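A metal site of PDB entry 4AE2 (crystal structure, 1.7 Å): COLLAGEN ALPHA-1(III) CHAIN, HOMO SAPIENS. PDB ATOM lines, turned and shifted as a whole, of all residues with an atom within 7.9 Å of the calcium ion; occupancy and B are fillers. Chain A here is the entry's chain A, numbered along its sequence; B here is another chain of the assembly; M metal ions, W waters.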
ATOM      1  N   PRO A  48     -14.747  -6.463  -5.431  1.00  0.00           N
ATOM      2  CA  PRO A  48     -15.874  -7.083  -6.127  1.00  0.00           C
ATOM      3  C   PRO A  48     -15.478  -7.667  -7.466  1.00  0.00           C
ATOM      4  O   PRO A  48     -14.541  -7.185  -8.107  1.00  0.00           O
ATOM      5  CB  PRO A  48     -16.852  -5.911  -6.325  1.00  0.00           C
ATOM      6  CG  PRO A  48     -15.999  -4.683  -6.306  1.00  0.00           C
ATOM      7  CD  PRO A  48     -14.849  -4.988  -5.383  1.00  0.00           C
ATOM      8  N   VAL A  69     -20.617  -7.497  -6.674  1.00  0.00           N
ATOM      9  CA  VAL A  69     -20.172  -7.371  -8.047  1.00  0.00           C
ATOM     10  C   VAL A  69     -20.244  -5.924  -8.490  1.00  0.00           C
ATOM     11  O   VAL A  69     -20.914  -5.108  -7.853  1.00  0.00           O
ATOM     12  CB  VAL A  69     -20.954  -8.289  -9.027  1.00  0.00           C
ATOM     13  CG1 VAL A  69     -20.792  -9.758  -8.604  1.00  0.00           C
ATOM     14  CG2 VAL A  69     -22.443  -7.893  -9.087  1.00  0.00           C
ATOM     15  N   ASP A  70     -19.537  -5.599  -9.565  1.00  0.00           N
ATOM     16  CA  ASP A  70     -19.393  -4.227  -9.997  1.00  0.00           C
ATOM     17  C   ASP A  70     -19.352  -4.188 -11.522  1.00  0.00           C
ATOM     18  O   ASP A  70     -18.283  -4.058 -12.128  1.00  0.00           O
ATOM     19  CB  ASP A  70     -18.119  -3.619  -9.394  1.00  0.00           C
ATOM     20  CG  ASP A  70     -17.994  -2.134  -9.655  1.00  0.00           C
ATOM     21  OD1 ASP A  70     -19.001  -1.484 -10.044  1.00  0.00           O
ATOM     22  OD2 ASP A  70     -16.884  -1.601  -9.471  1.00  0.00           O
ATOM     23  N   PRO A  71     -20.536  -4.293 -12.147  1.00  0.00           N
ATOM     24  CA  PRO A  71     -20.590  -4.441 -13.596  1.00  0.00           C
ATOM     25  C   PRO A  71     -19.886  -3.297 -14.349  1.00  0.00           C
ATOM     26  O   PRO A  71     -19.296  -3.549 -15.396  1.00  0.00           O
ATOM     27  CB  PRO A  71     -22.102  -4.508 -13.876  1.00  0.00           C
ATOM     28  CG  PRO A  71     -22.653  -5.169 -12.651  1.00  0.00           C
ATOM     29  CD  PRO A  71     -21.847  -4.563 -11.519  1.00  0.00           C
ATOM     30  N   ASN A  72     -19.912  -2.079 -13.799  1.00  0.00           N
ATOM     31  CA  ASN A  72     -19.327  -0.912 -14.498  1.00  0.00           C
ATOM     32  C   ASN A  72     -17.870  -0.694 -14.130  1.00  0.00           C
ATOM     33  O   ASN A  72     -17.233   0.266 -14.592  1.00  0.00           O
ATOM     34  CB  ASN A  72     -20.171   0.345 -14.284  1.00  0.00           C
ATOM     35  CG  ASN A  72     -20.062   0.895 -12.878  1.00  0.00           C
ATOM     36  OD1 ASN A  72     -19.221   0.473 -12.088  1.00  0.00           O
ATOM     37  ND2 ASN A  72     -20.896   1.873 -12.565  1.00  0.00           N
ATOM     38  N   GLN A  73     -17.340  -1.620 -13.315  1.00  0.00           N
ATOM     39  CA  GLN A  73     -15.909  -1.655 -12.962  1.00  0.00           C
ATOM     40  C   GLN A  73     -15.406  -0.290 -12.501  1.00  0.00           C
ATOM     41  O   GLN A  73     -16.139   0.422 -11.822  1.00  0.00           O
ATOM     42  CB  GLN A  73     -15.082  -2.272 -14.117  1.00  0.00           C
ATOM     43  CG  GLN A  73     -15.474  -3.719 -14.429  1.00  0.00           C
ATOM     44  CD  GLN A  73     -14.864  -4.701 -13.446  1.00  0.00           C
ATOM     45  OE1 GLN A  73     -15.491  -5.085 -12.451  1.00  0.00           O
ATOM     46  NE2 GLN A  73     -13.630  -5.090 -13.688  1.00  0.00           N
ATOM     47  N   GLY A  74     -14.180   0.091 -12.873  1.00  0.00           N
ATOM     48  CA  GLY A  74     -13.599   1.349 -12.379  1.00  0.00           C
ATOM     49  C   GLY A  74     -13.629   1.447 -10.864  1.00  0.00           C
ATOM     50  O   GLY A  74     -13.294   0.481 -10.181  1.00  0.00           O
ATOM     51  N   CYS A  75     -14.063   2.589 -10.340  1.00  0.00           N
ATOM     52  CA  CYS A  75     -14.202   2.801  -8.896  1.00  0.00           C
ATOM     53  C   CYS A  75     -15.138   1.748  -8.273  1.00  0.00           C
ATOM     54  O   CYS A  75     -16.227   1.458  -8.793  1.00  0.00           O
ATOM     55  CB  CYS A  75     -14.714   4.235  -8.628  1.00  0.00           C
ATOM     56  SG  CYS A  75     -14.926   4.715  -6.892  1.00  0.00           S
ATOM     57  N   LYS A  76     -14.686   1.155  -7.182  1.00  0.00           N
ATOM     58  CA  LYS A  76     -15.386   0.026  -6.539  1.00  0.00           C
ATOM     59  C   LYS A  76     -16.553   0.440  -5.638  1.00  0.00           C
ATOM     60  O   LYS A  76     -17.326  -0.414  -5.174  1.00  0.00           O
ATOM     61  CB  LYS A  76     -14.400  -0.793  -5.695  1.00  0.00           C
ATOM     62  CG  LYS A  76     -13.366  -1.586  -6.491  1.00  0.00           C
ATOM     63  N   LEU A  77     -16.706   1.739  -5.381  1.00  0.00           N
ATOM     64  CA  LEU A  77     -17.632   2.237  -4.350  1.00  0.00           C
ATOM     65  C   LEU A  77     -19.106   1.994  -4.662  1.00  0.00           C
ATOM     66  O   LEU A  77     -19.949   2.001  -3.760  1.00  0.00           O
ATOM     67  CB  LEU A  77     -17.384   3.723  -4.062  1.00  0.00           C
ATOM     68  CG  LEU A  77     -16.126   4.061  -3.275  1.00  0.00           C
ATOM     69  CD1 LEU A  77     -15.873   5.566  -3.332  1.00  0.00           C
ATOM     70  CD2 LEU A  77     -16.227   3.587  -1.836  1.00  0.00           C
ATOM     71  N   ASP A  78     -19.420   1.783  -5.937  1.00  0.00           N
ATOM     72  CA  ASP A  78     -20.806   1.539  -6.315  1.00  0.00           C
ATOM     73  C   ASP A  78     -21.094   0.058  -6.589  1.00  0.00           C
ATOM     74  O   ASP A  78     -22.076  -0.277  -7.248  1.00  0.00           O
ATOM     75  CB  ASP A  78     -21.208   2.415  -7.509  1.00  0.00           C
ATOM     76  CG  ASP A  78     -20.367   2.172  -8.764  1.00  0.00           C
ATOM     77  OD1 ASP A  78     -19.425   1.328  -8.744  1.00  0.00           O
ATOM     78  OD2 ASP A  78     -20.648   2.825  -9.769  1.00  0.00           O
ATOM     79  N   ALA A  79     -20.239  -0.835  -6.073  1.00  0.00           N
ATOM     80  CA  ALA A  79     -20.502  -2.273  -6.174  1.00  0.00           C
ATOM     81  C   ALA A  79     -21.858  -2.618  -5.539  1.00  0.00           C
ATOM     82  O   ALA A  79     -22.308  -1.942  -4.608  1.00  0.00           O
ATOM     83  CB  ALA A  79     -19.375  -3.102  -5.565  1.00  0.00           C
ATOM     84  N   ILE A  80     -22.515  -3.634  -6.076  1.00  0.00           N
ATOM     85  CA  ILE A  80     -23.833  -4.057  -5.585  1.00  0.00           C
ATOM     86  C   ILE A  80     -23.799  -5.478  -5.041  1.00  0.00           C
ATOM     87  O   ILE A  80     -23.018  -6.324  -5.486  1.00  0.00           O
ATOM     88  CB  ILE A  80     -24.920  -3.935  -6.677  1.00  0.00           C
ATOM     89  CG1 ILE A  80     -24.520  -4.702  -7.936  1.00  0.00           C
ATOM     90  CG2 ILE A  80     -25.228  -2.463  -6.968  1.00  0.00           C
ATOM     91  CD1 ILE A  80     -25.662  -4.922  -8.898  1.00  0.00           C
ATOM     92  N   VAL A 139     -27.363   5.334  -9.889  1.00  0.00           N
ATOM     93  CA  VAL A 139     -26.264   4.383  -9.821  1.00  0.00           C
ATOM     94  C   VAL A 139     -26.727   2.954 -10.135  1.00  0.00           C
ATOM     95  O   VAL A 139     -26.099   2.244 -10.930  1.00  0.00           O
ATOM     96  CB  VAL A 139     -25.535   4.427  -8.454  1.00  0.00           C
ATOM     97  CG1 VAL A 139     -24.543   3.288  -8.352  1.00  0.00           C
ATOM     98  CG2 VAL A 139     -24.842   5.775  -8.275  1.00  0.00           C
ATOM     99  N   GLN A 143     -25.637   0.271 -13.262  1.00  0.00           N
ATOM    100  CA  GLN A 143     -25.177  -1.083 -13.004  1.00  0.00           C
ATOM    101  C   GLN A 143     -26.101  -2.092 -13.668  1.00  0.00           C
ATOM    102  O   GLN A 143     -25.626  -3.016 -14.329  1.00  0.00           O
ATOM    103  CB  GLN A 143     -25.037  -1.345 -11.500  1.00  0.00           C
ATOM    104  CG  GLN A 143     -23.963  -0.480 -10.806  1.00  0.00           C
ATOM    105  CD  GLN A 143     -22.546  -0.950 -11.108  1.00  0.00           C
ATOM    106  OE1 GLN A 143     -22.205  -1.313 -12.259  1.00  0.00           O
ATOM    107  NE2 GLN A 143     -21.708  -0.978 -10.072  1.00  0.00           N
ATOM    108  N   ARG B  50     -12.039   6.224 -15.289  1.00  0.00           N
ATOM    109  CA  ARG B  50     -12.951   5.768 -16.340  1.00  0.00           C
ATOM    110  C   ARG B  50     -13.906   6.887 -16.788  1.00  0.00           C
ATOM    111  O   ARG B  50     -14.254   6.982 -17.970  1.00  0.00           O
ATOM    112  CB  ARG B  50     -13.724   4.540 -15.901  1.00  0.00           C
ATOM    113  CG  ARG B  50     -14.308   3.846 -17.097  1.00  0.00           C
ATOM    114  CD  ARG B  50     -15.042   2.555 -16.778  1.00  0.00           C
ATOM    115  NE  ARG B  50     -15.230   1.890 -18.062  1.00  0.00           N
ATOM    116  CZ  ARG B  50     -15.700   0.674 -18.233  1.00  0.00           C
ATOM    117  NH1 ARG B  50     -16.125  -0.033 -17.180  1.00  0.00           N
ATOM    118  NH2 ARG B  50     -15.775   0.177 -19.464  1.00  0.00           N
ATOM    119  N   ASP B  54     -16.542   8.493 -11.428  1.00  0.00           N
ATOM    120  CA  ASP B  54     -15.582   7.713 -10.665  1.00  0.00           C
ATOM    121  C   ASP B  54     -14.598   8.603  -9.919  1.00  0.00           C
ATOM    122  O   ASP B  54     -14.262   8.329  -8.768  1.00  0.00           O
ATOM    123  CB  ASP B  54     -14.843   6.731 -11.550  1.00  0.00           C
ATOM    124  CG  ASP B  54     -15.624   5.469 -11.807  1.00  0.00           C
ATOM    125  OD1 ASP B  54     -16.804   5.381 -11.401  1.00  0.00           O
ATOM    126  OD2 ASP B  54     -15.036   4.548 -12.413  1.00  0.00           O
ATOM    127  N   CYS B  58     -14.357   8.305  -5.911  1.00  0.00           N
ATOM    128  CA  CYS B  58     -13.119   7.692  -5.454  1.00  0.00           C
ATOM    129  C   CYS B  58     -12.068   8.745  -5.044  1.00  0.00           C
ATOM    130  O   CYS B  58     -11.145   8.412  -4.310  1.00  0.00           O
ATOM    131  CB  CYS B  58     -12.568   6.718  -6.501  1.00  0.00           C
ATOM    132  SG  CYS B  58     -13.017   4.967  -6.222  1.00  0.00           S
ATOM    133  N   LEU B 150     -22.026   4.176 -19.401  1.00  0.00           N
ATOM    134  CA  LEU B 150     -21.696   4.539 -18.030  1.00  0.00           C
ATOM    135  C   LEU B 150     -22.594   5.620 -17.422  1.00  0.00           C
ATOM    136  O   LEU B 150     -22.478   5.903 -16.232  1.00  0.00           O
ATOM    137  CB  LEU B 150     -20.238   5.028 -17.979  1.00  0.00           C
ATOM    138  CG  LEU B 150     -19.164   3.957 -18.195  1.00  0.00           C
ATOM    139  CD1 LEU B 150     -17.847   4.574 -18.682  1.00  0.00           C
ATOM    140  CD2 LEU B 150     -18.962   3.135 -16.926  1.00  0.00           C
HETATM  141 CA    CA M   1     -17.800   0.661 -10.275  1.00  0.00          CA
HETATM  142  O   HOH W   1     -17.949   3.025 -10.831  1.00  0.00           O
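The backbone NH (N) of Cys 75 lies within hydrogen-bond range of the side-chain carboxylate (OD2) of Asp 54 of chain B (3.0 Å).
SG of Cys 75 sits close to N of Leu 77, 3.8 Å away.
The side-chain sulfur (SG) of Cys 75 forms a disulfide with the side-chain sulfur (SG) of Cys 58 of chain B (2.0 Å).
N of Asn 72 is in hydrogen-bond range of OE1 of Gln 143 (2.9 Å).
The backbone carbonyl oxygen (O) of Asn 72 lies within hydrogen-bond range of the guanidinium group (NH1) of Arg 50 of chain B, 2.8 Å away.
The backbone carbonyl oxygen of Asp 78 is in hydrogen-bond range of the side-chain amide nitrogen of Gln 143 (2.9 Å).
OD1 of Asp 70 sits close to NE2 of Gln 143 (2.8 Å).
Water W1 bridges OD1 of Asp 54 of chain B (2.7 Å) and OD2 of Asp 78 (2.9 Å).
The calcium ion is bound by O of Gln 73, O of Cys 75, OD1 of Asn 72, OD1 of Asp 78, water W1, OD1 of Asp 70 and OD2 of Asp 70.
Within 4 Å of the calcium ion: Asp 70, Asn 72, Gln 73, Cys 75 and Asp 78.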
